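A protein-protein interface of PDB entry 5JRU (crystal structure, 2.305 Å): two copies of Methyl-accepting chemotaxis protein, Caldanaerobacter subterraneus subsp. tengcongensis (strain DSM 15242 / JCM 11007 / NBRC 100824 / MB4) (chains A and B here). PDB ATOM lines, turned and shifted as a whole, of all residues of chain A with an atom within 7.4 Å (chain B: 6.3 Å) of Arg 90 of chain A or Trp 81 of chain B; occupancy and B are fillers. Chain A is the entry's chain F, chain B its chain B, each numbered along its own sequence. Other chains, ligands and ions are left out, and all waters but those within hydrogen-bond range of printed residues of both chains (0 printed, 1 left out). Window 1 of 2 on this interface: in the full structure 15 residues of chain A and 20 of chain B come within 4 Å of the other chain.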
ATOM      1  N   PHE A  86       9.646  16.899  -1.369  1.00  0.00           N
ATOM      2  CA  PHE A  86      10.219  16.947  -0.028  1.00  0.00           C
ATOM      3  C   PHE A  86       9.320  17.711   0.949  1.00  0.00           C
ATOM      4  O   PHE A  86       9.252  17.353   2.128  1.00  0.00           O
ATOM      5  CB  PHE A  86      11.599  17.592  -0.062  1.00  0.00           C
ATOM      6  CG  PHE A  86      12.652  16.764  -0.756  1.00  0.00           C
ATOM      7  CD1 PHE A  86      12.711  16.713  -2.150  1.00  0.00           C
ATOM      8  CD2 PHE A  86      13.602  16.064  -0.023  1.00  0.00           C
ATOM      9  CE1 PHE A  86      13.688  15.959  -2.805  1.00  0.00           C
ATOM     10  CE2 PHE A  86      14.587  15.312  -0.670  1.00  0.00           C
ATOM     11  CZ  PHE A  86      14.632  15.269  -2.059  1.00  0.00           C
ATOM     12  N   ALA A  87       8.638  18.749   0.457  1.00  0.00           N
ATOM     13  CA  ALA A  87       7.899  19.671   1.325  1.00  0.00           C
ATOM     14  C   ALA A  87       6.880  18.972   2.241  1.00  0.00           C
ATOM     15  O   ALA A  87       6.122  18.097   1.813  1.00  0.00           O
ATOM     16  CB  ALA A  87       7.180  20.734   0.485  1.00  0.00           C
ATOM     17  N   GLY A  88       6.885  19.361   3.511  1.00  0.00           N
ATOM     18  CA  GLY A  88       5.926  18.859   4.484  1.00  0.00           C
ATOM     19  C   GLY A  88       5.915  17.372   4.799  1.00  0.00           C
ATOM     20  O   GLY A  88       4.971  16.891   5.427  1.00  0.00           O
ATOM     21  N   ARG A  89       6.972  16.651   4.437  1.00  0.00           N
ATOM     22  CA  ARG A  89       7.053  15.208   4.687  1.00  0.00           C
ATOM     23  C   ARG A  89       7.819  14.891   5.967  1.00  0.00           C
ATOM     24  O   ARG A  89       8.710  15.620   6.358  1.00  0.00           O
ATOM     25  CB  ARG A  89       7.791  14.485   3.541  1.00  0.00           C
ATOM     26  CG  ARG A  89       6.977  13.867   2.434  1.00  0.00           C
ATOM     27  CD  ARG A  89       6.603  14.947   1.485  1.00  0.00           C
ATOM     28  NE  ARG A  89       6.028  14.474   0.236  1.00  0.00           N
ATOM     29  CZ  ARG A  89       5.327  15.259  -0.575  1.00  0.00           C
ATOM     30  NH1 ARG A  89       5.110  16.522  -0.214  1.00  0.00           N
ATOM     31  NH2 ARG A  89       4.838  14.789  -1.724  1.00  0.00           N
ATOM     32  N   ARG A  90       7.450  13.795   6.612  1.00  0.00           N
ATOM     33  CA  ARG A  90       8.298  13.162   7.612  1.00  0.00           C
ATOM     34  C   ARG A  90       9.297  12.319   6.837  1.00  0.00           C
ATOM     35  O   ARG A  90       9.006  11.903   5.712  1.00  0.00           O
ATOM     36  CB  ARG A  90       7.462  12.312   8.556  1.00  0.00           C
ATOM     37  CG  ARG A  90       6.303  13.056   9.171  1.00  0.00           C
ATOM     38  CD  ARG A  90       5.407  12.087   9.917  1.00  0.00           C
ATOM     39  NE  ARG A  90       6.113  11.272  10.894  1.00  0.00           N
ATOM     40  CZ  ARG A  90       5.646  10.129  11.384  1.00  0.00           C
ATOM     41  NH1 ARG A  90       4.486   9.650  10.935  1.00  0.00           N
ATOM     42  NH2 ARG A  90       6.364   9.432  12.266  1.00  0.00           N
ATOM     43  N   LEU A  91      10.445  12.021   7.428  1.00  0.00           N
ATOM     44  CA  LEU A  91      11.431  11.224   6.717  1.00  0.00           C
ATOM     45  C   LEU A  91      10.804   9.929   6.247  1.00  0.00           C
ATOM     46  O   LEU A  91      10.853   9.604   5.075  1.00  0.00           O
ATOM     47  CB  LEU A  91      12.640  10.945   7.605  1.00  0.00           C
ATOM     48  CG  LEU A  91      13.687   9.996   7.004  1.00  0.00           C
ATOM     49  CD1 LEU A  91      14.362  10.541   5.733  1.00  0.00           C
ATOM     50  CD2 LEU A  91      14.730   9.637   8.060  1.00  0.00           C
ATOM     51  N   VAL A  92      10.124   9.246   7.160  1.00  0.00           N
ATOM     52  CA  VAL A  92       9.524   7.955   6.853  1.00  0.00           C
ATOM     53  C   VAL A  92       8.475   8.083   5.720  1.00  0.00           C
ATOM     54  O   VAL A  92       8.363   7.180   4.869  1.00  0.00           O
ATOM     55  CB  VAL A  92       8.894   7.310   8.138  1.00  0.00           C
ATOM     56  CG1 VAL A  92       7.681   8.113   8.662  1.00  0.00           C
ATOM     57  CG2 VAL A  92       8.491   5.881   7.884  1.00  0.00           C
ATOM     58  N   ASN A  93       7.750   9.209   5.667  1.00  0.00           N
ATOM     59  CA  ASN A  93       6.857   9.453   4.528  1.00  0.00           C
ATOM     60  C   ASN A  93       7.680   9.454   3.242  1.00  0.00           C
ATOM     61  O   ASN A  93       7.347   8.781   2.263  1.00  0.00           O
ATOM     62  CB  ASN A  93       6.137  10.805   4.616  1.00  0.00           C
ATOM     63  CG  ASN A  93       5.200  10.914   5.772  1.00  0.00           C
ATOM     64  OD1 ASN A  93       4.966  12.019   6.251  1.00  0.00           O
ATOM     65  ND2 ASN A  93       4.633   9.784   6.228  1.00  0.00           N
ATOM     66  N   PHE A  94       8.750  10.242   3.260  1.00  0.00           N
ATOM     67  CA  PHE A  94       9.585  10.421   2.074  1.00  0.00           C
ATOM     68  C   PHE A  94      10.085   9.076   1.534  1.00  0.00           C
ATOM     69  O   PHE A  94       9.986   8.796   0.340  1.00  0.00           O
ATOM     70  CB  PHE A  94      10.766  11.355   2.377  1.00  0.00           C
ATOM     71  CG  PHE A  94      11.645  11.637   1.189  1.00  0.00           C
ATOM     72  CD1 PHE A  94      11.221  12.514   0.184  1.00  0.00           C
ATOM     73  CD2 PHE A  94      12.898  11.042   1.066  1.00  0.00           C
ATOM     74  CE1 PHE A  94      12.034  12.792  -0.911  1.00  0.00           C
ATOM     75  CE2 PHE A  94      13.708  11.317  -0.052  1.00  0.00           C
ATOM     76  CZ  PHE A  94      13.269  12.201  -1.028  1.00  0.00           C
ATOM     77  N   LEU A  95      10.595   8.239   2.422  1.00  0.00           N
ATOM     78  CA  LEU A  95      11.109   6.922   2.029  1.00  0.00           C
ATOM     79  C   LEU A  95       9.990   5.977   1.549  1.00  0.00           C
ATOM     80  O   LEU A  95      10.147   5.260   0.565  1.00  0.00           O
ATOM     81  CB  LEU A  95      11.846   6.314   3.200  1.00  0.00           C
ATOM     82  CG  LEU A  95      13.060   7.119   3.680  1.00  0.00           C
ATOM     83  CD1 LEU A  95      13.679   6.409   4.873  1.00  0.00           C
ATOM     84  CD2 LEU A  95      14.115   7.315   2.564  1.00  0.00           C
ATOM     85  N   MET A  96       8.844   6.007   2.233  1.00  0.00           N
ATOM     86  CA  MET A  96       7.761   5.131   1.852  1.00  0.00           C
ATOM     87  C   MET A  96       7.134   5.542   0.536  1.00  0.00           C
ATOM     88  O   MET A  96       6.649   4.698  -0.204  1.00  0.00           O
ATOM     89  CB  MET A  96       6.732   5.087   2.954  1.00  0.00           C
ATOM     90  CG  MET A  96       7.213   4.163   4.068  1.00  0.00           C
ATOM     91  SD  MET A  96       6.149   4.145   5.524  1.00  0.00           S
ATOM     92  CE  MET A  96       4.599   3.619   4.762  1.00  0.00           C
ATOM     93  N   MET A  97       7.224   6.827   0.214  1.00  0.00           N
ATOM     94  CA  MET A  97       6.658   7.386  -1.017  1.00  0.00           C
ATOM     95  C   MET A  97       7.611   7.315  -2.212  1.00  0.00           C
ATOM     96  O   MET A  97       7.222   7.572  -3.346  1.00  0.00           O
ATOM     97  CB  MET A  97       6.252   8.855  -0.780  1.00  0.00           C
ATOM     98  CG  MET A  97       5.004   9.068   0.116  1.00  0.00           C
ATOM     99  SD  MET A  97       4.751  10.752   0.724  1.00  0.00           S
ATOM    100  CE  MET A  97       3.118  10.600   1.514  1.00  0.00           C
ATOM    101  N   PHE A 152      16.067  15.612   6.475  1.00  0.00           N
ATOM    102  CA  PHE A 152      14.887  15.751   7.329  1.00  0.00           C
ATOM    103  C   PHE A 152      15.256  15.912   8.800  1.00  0.00           C
ATOM    104  O   PHE A 152      14.384  16.149   9.633  1.00  0.00           O
ATOM    105  CB  PHE A 152      13.949  14.554   7.123  1.00  0.00           C
ATOM    106  CG  PHE A 152      13.244  14.606   5.812  1.00  0.00           C
ATOM    107  CD1 PHE A 152      12.097  15.383   5.652  1.00  0.00           C
ATOM    108  CD2 PHE A 152      13.776  13.932   4.700  1.00  0.00           C
ATOM    109  CE1 PHE A 152      11.457  15.474   4.397  1.00  0.00           C
ATOM    110  CE2 PHE A 152      13.148  13.985   3.461  1.00  0.00           C
ATOM    111  CZ  PHE A 152      11.986  14.771   3.296  1.00  0.00           C
ATOM    112  N   GLU A 154      16.129  13.736  10.984  1.00  0.00           N
ATOM    113  CA  GLU A 154      15.588  12.637  11.763  1.00  0.00           C
ATOM    114  C   GLU A 154      16.651  11.559  11.790  1.00  0.00           C
ATOM    115  O   GLU A 154      17.132  11.104  10.753  1.00  0.00           O
ATOM    116  CB  GLU A 154      14.280  12.113  11.184  1.00  0.00           C
ATOM    117  CG  GLU A 154      13.180  13.162  11.135  1.00  0.00           C
ATOM    118  CD  GLU A 154      11.832  12.571  10.757  1.00  0.00           C
ATOM    119  OE1 GLU A 154      11.448  11.533  11.344  1.00  0.00           O
ATOM    120  OE2 GLU A 154      11.123  13.174   9.927  1.00  0.00           O
ATOM    121  N   PHE A 178      13.669   4.318  13.371  1.00  0.00           N
ATOM    122  CA  PHE A 178      13.473   5.729  13.712  1.00  0.00           C
ATOM    123  C   PHE A 178      13.377   5.938  15.234  1.00  0.00           C
ATOM    124  O   PHE A 178      13.144   4.994  15.996  1.00  0.00           O
ATOM    125  CB  PHE A 178      12.206   6.284  13.039  1.00  0.00           C
ATOM    126  CG  PHE A 178      12.176   6.104  11.547  1.00  0.00           C
ATOM    127  CD1 PHE A 178      11.766   4.905  10.979  1.00  0.00           C
ATOM    128  CD2 PHE A 178      12.541   7.142  10.717  1.00  0.00           C
ATOM    129  CE1 PHE A 178      11.727   4.757   9.623  1.00  0.00           C
ATOM    130  CE2 PHE A 178      12.511   6.987   9.356  1.00  0.00           C
ATOM    131  CZ  PHE A 178      12.104   5.789   8.807  1.00  0.00           C
ATOM    132  N   ASN A 180      10.970   7.737  16.681  1.00  0.00           N
ATOM    133  CA  ASN A 180       9.534   7.824  17.028  1.00  0.00           C
ATOM    134  C   ASN A 180       8.703   6.832  16.228  1.00  0.00           C
ATOM    135  O   ASN A 180       9.123   6.397  15.165  1.00  0.00           O
ATOM    136  CB  ASN A 180       9.019   9.245  16.810  1.00  0.00           C
ATOM    137  CG  ASN A 180       9.837  10.279  17.578  1.00  0.00           C
ATOM    138  OD1 ASN A 180      10.821  10.817  17.063  1.00  0.00           O
ATOM    139  ND2 ASN A 180       9.448  10.542  18.820  1.00  0.00           N
ATOM    140  N   PRO A 181       7.504   6.484  16.703  1.00  0.00           N
ATOM    141  CA  PRO A 181       6.734   5.523  15.901  1.00  0.00           C
ATOM    142  C   PRO A 181       6.375   5.974  14.467  1.00  0.00           C
ATOM    143  O   PRO A 181       6.262   7.174  14.155  1.00  0.00           O
ATOM    144  CB  PRO A 181       5.454   5.340  16.722  1.00  0.00           C
ATOM    145  CG  PRO A 181       5.846   5.703  18.117  1.00  0.00           C
ATOM    146  CD  PRO A 181       6.827   6.823  17.961  1.00  0.00           C
ATOM    147  N   VAL A 182       6.255   4.982  13.587  1.00  0.00           N
ATOM    148  CA  VAL A 182       5.850   5.213  12.209  1.00  0.00           C
ATOM    149  C   VAL A 182       4.435   5.742  12.196  1.00  0.00           C
ATOM    150  O   VAL A 182       4.149   6.727  11.548  1.00  0.00           O
ATOM    151  CB  VAL A 182       5.914   3.933  11.350  1.00  0.00           C
ATOM    152  CG1 VAL A 182       5.402   4.225   9.923  1.00  0.00           C
ATOM    153  CG2 VAL A 182       7.344   3.348  11.335  1.00  0.00           C
ATOM    154  N   PHE A 183       3.543   5.058  12.902  1.00  0.00           N
ATOM    155  CA  PHE A 183       2.166   5.519  13.023  1.00  0.00           C
ATOM    156  C   PHE A 183       1.820   5.808  14.456  1.00  0.00           C
ATOM    157  O   PHE A 183       1.014   5.124  15.059  1.00  0.00           O
ATOM    158  CB  PHE A 183       1.214   4.483  12.451  1.00  0.00           C
ATOM    159  CG  PHE A 183       1.516   4.129  11.043  1.00  0.00           C
ATOM    160  CD1 PHE A 183       1.291   5.043  10.033  1.00  0.00           C
ATOM    161  CD2 PHE A 183       2.115   2.929  10.735  1.00  0.00           C
ATOM    162  CE1 PHE A 183       1.575   4.734   8.734  1.00  0.00           C
ATOM    163  CE2 PHE A 183       2.426   2.618   9.446  1.00  0.00           C
ATOM    164  CZ  PHE A 183       2.153   3.524   8.434  1.00  0.00           C
ATOM    165  N   GLU A 184       2.379   6.878  14.983  1.00  0.00           N
ATOM    166  CA  GLU A 184       2.160   7.181  16.376  1.00  0.00           C
ATOM    167  C   GLU A 184       0.735   7.646  16.643  1.00  0.00           C
ATOM    168  O   GLU A 184       0.182   8.459  15.908  1.00  0.00           O
ATOM    169  CB  GLU A 184       3.151   8.260  16.824  1.00  0.00           C
ATOM    170  CG  GLU A 184       3.044   8.608  18.278  1.00  0.00           C
ATOM    171  CD  GLU A 184       4.145   9.545  18.725  1.00  0.00           C
ATOM    172  OE1 GLU A 184       4.720  10.261  17.867  1.00  0.00           O
ATOM    173  OE2 GLU A 184       4.433   9.559  19.941  1.00  0.00           O
ATOM    174  N   TYR A 185       0.124   7.087  17.679  1.00  0.00           N
ATOM    175  CA  TYR A 185      -1.061   7.698  18.247  1.00  0.00           C
ATOM    176  C   TYR A 185      -0.612   8.540  19.420  1.00  0.00           C
ATOM    177  O   TYR A 185       0.051   8.030  20.321  1.00  0.00           O
ATOM    178  CB  TYR A 185      -2.086   6.670  18.713  1.00  0.00           C
ATOM    179  CG  TYR A 185      -3.312   7.332  19.332  1.00  0.00           C
ATOM    180  CD1 TYR A 185      -4.459   7.562  18.580  1.00  0.00           C
ATOM    181  CD2 TYR A 185      -3.310   7.754  20.664  1.00  0.00           C
ATOM    182  CE1 TYR A 185      -5.560   8.181  19.130  1.00  0.00           C
ATOM    183  CE2 TYR A 185      -4.411   8.379  21.222  1.00  0.00           C
ATOM    184  CZ  TYR A 185      -5.536   8.588  20.452  1.00  0.00           C
ATOM    185  OH  TYR A 185      -6.643   9.207  21.000  1.00  0.00           O
ATOM    186  N   LYS A 186      -0.960   9.818  19.431  1.00  0.00           N
ATOM    187  CA  LYS A 186      -0.622  10.633  20.583  1.00  0.00           C
ATOM    188  C   LYS A 186      -1.881  11.318  21.120  1.00  0.00           C
ATOM    189  O   LYS A 186      -2.974  11.163  20.554  1.00  0.00           O
ATOM    190  CB  LYS A 186       0.458  11.655  20.210  1.00  0.00           C
ATOM    191  CG  LYS A 186       0.044  12.597  19.083  1.00  0.00           C
ATOM    192  CD  LYS A 186       1.152  13.585  18.671  1.00  0.00           C
ATOM    193  CE  LYS A 186       2.509  12.916  18.495  1.00  0.00           C
ATOM    194  NZ  LYS A 186       3.259  13.526  17.352  1.00  0.00           N
ATOM    195  N   THR B   4      -2.272  -1.440  11.770  1.00  0.00           N
ATOM    196  CA  THR B   4      -2.009  -0.009  11.840  1.00  0.00           C
ATOM    197  C   THR B   4      -3.197   0.756  12.395  1.00  0.00           C
ATOM    198  O   THR B   4      -3.091   1.443  13.412  1.00  0.00           O
ATOM    199  CB  THR B   4      -1.741   0.608  10.445  1.00  0.00           C
ATOM    200  OG1 THR B   4      -0.565   0.045   9.847  1.00  0.00           O
ATOM    201  CG2 THR B   4      -1.600   2.107  10.558  1.00  0.00           C
ATOM    202  N   ILE B   5      -4.347   0.557  11.753  1.00  0.00           N
ATOM    203  CA  ILE B   5      -5.515   1.330  12.091  1.00  0.00           C
ATOM    204  C   ILE B   5      -6.117   0.743  13.352  1.00  0.00           C
ATOM    205  O   ILE B   5      -6.694   1.494  14.142  1.00  0.00           O
ATOM    206  CB  ILE B   5      -6.553   1.392  10.950  1.00  0.00           C
ATOM    207  CG1 ILE B   5      -7.663   2.401  11.272  1.00  0.00           C
ATOM    208  CG2 ILE B   5      -7.188   0.084  10.730  1.00  0.00           C
ATOM    209  CD1 ILE B   5      -8.534   2.843  10.038  1.00  0.00           C
ATOM    210  N   THR B   8      -4.439   2.035  16.483  1.00  0.00           N
ATOM    211  CA  THR B   8      -4.981   3.364  16.715  1.00  0.00           C
ATOM    212  C   THR B   8      -6.401   3.342  17.351  1.00  0.00           C
ATOM    213  O   THR B   8      -6.668   4.090  18.286  1.00  0.00           O
ATOM    214  CB  THR B   8      -4.999   4.118  15.397  1.00  0.00           C
ATOM    215  OG1 THR B   8      -3.643   4.289  14.977  1.00  0.00           O
ATOM    216  CG2 THR B   8      -5.698   5.468  15.526  1.00  0.00           C
ATOM    217  N   LYS B  76      -7.149  13.726  13.198  1.00  0.00           N
ATOM    218  CA  LYS B  76      -5.950  14.319  13.783  1.00  0.00           C
ATOM    219  C   LYS B  76      -4.745  13.379  13.711  1.00  0.00           C
ATOM    220  O   LYS B  76      -3.643  13.746  13.303  1.00  0.00           O
ATOM    221  CB  LYS B  76      -6.213  14.679  15.251  1.00  0.00           C
ATOM    222  CG  LYS B  76      -5.016  15.295  15.980  1.00  0.00           C
ATOM    223  CD  LYS B  76      -5.351  15.587  17.468  1.00  0.00           C
ATOM    224  CE  LYS B  76      -4.115  15.986  18.315  1.00  0.00           C
ATOM    225  NZ  LYS B  76      -3.130  14.887  18.585  1.00  0.00           N
ATOM    226  N   THR B  77      -5.011  12.136  14.050  1.00  0.00           N
ATOM    227  CA  THR B  77      -4.004  11.107  14.021  1.00  0.00           C
ATOM    228  C   THR B  77      -3.431  10.888  12.617  1.00  0.00           C
ATOM    229  O   THR B  77      -2.220  10.847  12.452  1.00  0.00           O
ATOM    230  CB  THR B  77      -4.593   9.818  14.525  1.00  0.00           C
ATOM    231  OG1 THR B  77      -5.151  10.048  15.830  1.00  0.00           O
ATOM    232  CG2 THR B  77      -3.522   8.752  14.555  1.00  0.00           C
ATOM    233  N   PHE B  78      -4.307  10.789  11.614  1.00  0.00           N
ATOM    234  CA  PHE B  78      -3.875  10.622  10.217  1.00  0.00           C
ATOM    235  C   PHE B  78      -3.008  11.781   9.758  1.00  0.00           C
ATOM    236  O   PHE B  78      -2.090  11.604   8.942  1.00  0.00           O
ATOM    237  CB  PHE B  78      -5.078  10.517   9.272  1.00  0.00           C
ATOM    238  CG  PHE B  78      -5.916   9.285   9.465  1.00  0.00           C
ATOM    239  CD1 PHE B  78      -5.402   8.163  10.089  1.00  0.00           C
ATOM    240  CD2 PHE B  78      -7.247   9.258   9.011  1.00  0.00           C
ATOM    241  CE1 PHE B  78      -6.191   7.022  10.247  1.00  0.00           C
ATOM    242  CE2 PHE B  78      -8.046   8.123   9.166  1.00  0.00           C
ATOM    243  CZ  PHE B  78      -7.537   7.016   9.780  1.00  0.00           C
ATOM    244  N   SER B  79      -3.341  12.978  10.245  1.00  0.00           N
ATOM    245  CA  SER B  79      -2.593  14.178   9.863  1.00  0.00           C
ATOM    246  C   SER B  79      -1.218  14.190  10.490  1.00  0.00           C
ATOM    247  O   SER B  79      -0.305  14.844   9.973  1.00  0.00           O
ATOM    248  CB  SER B  79      -3.357  15.470  10.197  1.00  0.00           C
ATOM    249  OG  SER B  79      -3.333  15.777  11.561  1.00  0.00           O
ATOM    250  N   GLU B  80      -1.055  13.457  11.585  1.00  0.00           N
ATOM    251  CA  GLU B  80       0.281  13.298  12.149  1.00  0.00           C
ATOM    252  C   GLU B  80       1.068  12.237  11.371  1.00  0.00           C
ATOM    253  O   GLU B  80       2.265  12.404  11.160  1.00  0.00           O
ATOM    254  CB  GLU B  80       0.201  12.952  13.638  1.00  0.00           C
ATOM    255  CG  GLU B  80      -0.340  14.103  14.476  1.00  0.00           C
ATOM    256  CD  GLU B  80      -1.047  13.638  15.747  1.00  0.00           C
ATOM    257  OE1 GLU B  80      -1.174  12.420  15.976  1.00  0.00           O
ATOM    258  OE2 GLU B  80      -1.520  14.508  16.499  1.00  0.00           O
ATOM    259  N   TRP B  81       0.391  11.179  10.914  1.00  0.00           N
ATOM    260  CA  TRP B  81       1.029  10.144  10.087  1.00  0.00           C
ATOM    261  C   TRP B  81       1.486  10.671   8.733  1.00  0.00           C
ATOM    262  O   TRP B  81       2.617  10.430   8.293  1.00  0.00           O
ATOM    263  CB  TRP B  81       0.091   8.995   9.825  1.00  0.00           C
ATOM    264  CG  TRP B  81      -0.365   8.287  11.004  1.00  0.00           C
ATOM    265  CD1 TRP B  81       0.009   8.501  12.295  1.00  0.00           C
ATOM    266  CD2 TRP B  81      -1.308   7.213  11.030  1.00  0.00           C
ATOM    267  NE1 TRP B  81      -0.641   7.626  13.119  1.00  0.00           N
ATOM    268  CE2 TRP B  81      -1.455   6.822  12.366  1.00  0.00           C
ATOM    269  CE3 TRP B  81      -2.043   6.543  10.047  1.00  0.00           C
ATOM    270  CZ2 TRP B  81      -2.312   5.806  12.753  1.00  0.00           C
ATOM    271  CZ3 TRP B  81      -2.898   5.514  10.442  1.00  0.00           C
ATOM    272  CH2 TRP B  81      -3.009   5.153  11.778  1.00  0.00           C
ATOM    273  N   PHE B  82       0.582  11.367   8.052  1.00  0.00           N
ATOM    274  CA  PHE B  82       0.863  11.787   6.681  1.00  0.00           C
ATOM    275  C   PHE B  82       0.444  13.239   6.493  1.00  0.00           C
ATOM    276  O   PHE B  82      -0.555  13.527   5.818  1.00  0.00           O
ATOM    277  CB  PHE B  82       0.116  10.916   5.665  1.00  0.00           C
ATOM    278  CG  PHE B  82       0.520   9.476   5.654  1.00  0.00           C
ATOM    279  CD1 PHE B  82       1.630   9.052   4.906  1.00  0.00           C
ATOM    280  CD2 PHE B  82      -0.213   8.522   6.332  1.00  0.00           C
ATOM    281  CE1 PHE B  82       2.003   7.701   4.859  1.00  0.00           C
ATOM    282  CE2 PHE B  82       0.170   7.159   6.308  1.00  0.00           C
ATOM    283  CZ  PHE B  82       1.256   6.752   5.564  1.00  0.00           C
ATOM    284  N   PRO B  83       1.204  14.159   7.089  1.00  0.00           N
ATOM    285  CA  PRO B  83       0.857  15.585   7.057  1.00  0.00           C
ATOM    286  C   PRO B  83       0.765  16.158   5.636  1.00  0.00           C
ATOM    287  O   PRO B  83       0.017  17.130   5.424  1.00  0.00           O
ATOM    288  CB  PRO B  83       2.005  16.249   7.832  1.00  0.00           C
ATOM    289  CG  PRO B  83       3.168  15.192   7.824  1.00  0.00           C
ATOM    290  CD  PRO B  83       2.480  13.876   7.786  1.00  0.00           C
ATOM    291  N   ILE B 109       0.765   0.435   2.356  1.00  0.00           N
ATOM    292  CA  ILE B 109       0.438  -0.431   3.489  1.00  0.00           C
ATOM    293  C   ILE B 109      -0.154  -1.696   2.919  1.00  0.00           C
ATOM    294  O   ILE B 109      -1.383  -1.790   2.676  1.00  0.00           O
ATOM    295  CB  ILE B 109      -0.507   0.265   4.462  1.00  0.00           C
ATOM    296  CG1 ILE B 109       0.125   1.593   4.900  1.00  0.00           C
ATOM    297  CG2 ILE B 109      -0.797  -0.642   5.649  1.00  0.00           C
ATOM    298  CD1 ILE B 109      -0.687   2.417   5.869  1.00  0.00           C
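Among the printed residues, pairs that only touch across the chains: Gly 88 of chain A with Pro 83 of chain B (3.4 Å), Arg 90 of chain A with Glu 80 of chain B (3.4 Å), Asn 93 of chain A with Phe 82 of chain B (3.4 Å), Asn 93 of chain A with Pro 83 of chain B (3.5 Å), Phe 183 of chain A with Thr 4 of chain B (3.7 Å), Phe 183 of chain A with Trp 81 of chain B (3.3 Å), Phe 183 of chain A with Phe 82 of chain B (3.7 Å), Phe 183 of chain A with Ile 109 of chain B (3.98 Å), Glu 184 of chain A with Thr 77 of chain B (3.95 Å), Tyr 185 of chain A with Thr 8 of chain B (3.9 Å), Tyr 185 of chain A with Thr 77 of chain B (3.8 Å), Lys 186 of chain A with Lys 76 of chain B (3.9 Å) and Lys 186 of chain A with Glu 80 of chain B (3.3 Å).
OG1 of Thr 8 of chain B sits at hydrogen-bond distance from O of Thr 4 of chain B.
The side-chain carboxylate of Glu 184 of chain A is in salt-bridge range of the side-chain amino group of Lys 186 of chain A (3.6 Å).
The guanidinium group (NH2) of Arg 90 of chain A sits at hydrogen-bond distance from the backbone carbonyl oxygen (O) of Pro 181 of chain A.
The guanidinium group (NH1) of Arg 90 of chain A sits at hydrogen-bond distance from the backbone carbonyl oxygen (O) of Val 182 of chain A.
The side-chain amide oxygen (OD1) of Asn 93 of chain A sits at hydrogen-bond distance from the backbone NH (N) of Arg 90 of chain A, at 3.1 Å.
The backbone carbonyl oxygen (O) of Lys 76 of chain B lies within hydrogen-bond range of the side-chain hydroxyl (OG) of Ser 79 of chain B (2.7 Å).
No position is printed for both chains.
Of the 16 pairs that touch across the chains among the printed residues, none has its exchanged pair printed and touching as well.
Of the 22 printed residues of chain A, 7 touch a printed residue of chain B.
Of the 12 printed residues of chain B, 9 touch a printed residue of chain A.
Hydrophobic or aromatic side chains of chain B within 4 Å of the printed part of chain A: Trp 81, Phe 82, Pro 83 and Ile 109.
Among the printed residues, no Asp or Glu carboxylate lies within 4 Å of a Lys or Arg side-chain nitrogen of the other chain.
The backbone carbonyl oxygen (O) of Trp 81 of chain B lies within hydrogen-bond range of the guanidinium group (NH1) of Arg 90 of chain A (3.3 Å).
The indole nitrogen (NE1) of Trp 81 of chain B is in hydrogen-bond range of the backbone carbonyl oxygen (O) of Glu 184 of chain A (3.0 Å).
The backbone carbonyl oxygen (O) of Trp 81 of chain B lies within hydrogen-bond range of the side-chain amide nitrogen (ND2) of Asn 93 of chain A (3.0 Å).
Arg 90 of chain A touches just these residues of chain B: Glu 80 (3.4 Å) and Trp 81 (3.3 Å).
Of chain A, only Arg 90, Asn 93, Phe 183 and Glu 184 come within 4 Å of Trp 81 of chain B.
Of the printed residues of chain A, Lys 76 of chain B touches Lys 186.
Printed residues of chain B within 4 Å of Tyr 185 of chain A: Thr 8 (3.9 Å) and Thr 77 (3.8 Å).
Phe 86 of chain A touches none of the printed residues of chain B.
Phe 78 of chain B touches none of the printed residues of chain A.
The nearest residue of chain A that does not touch Trp 81 of chain B is Val 182 of chain A (4.6 Å).
The nearest printed residue of chain A that does not touch Phe 82 of chain B is Met 97 of chain A (4.01 Å).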
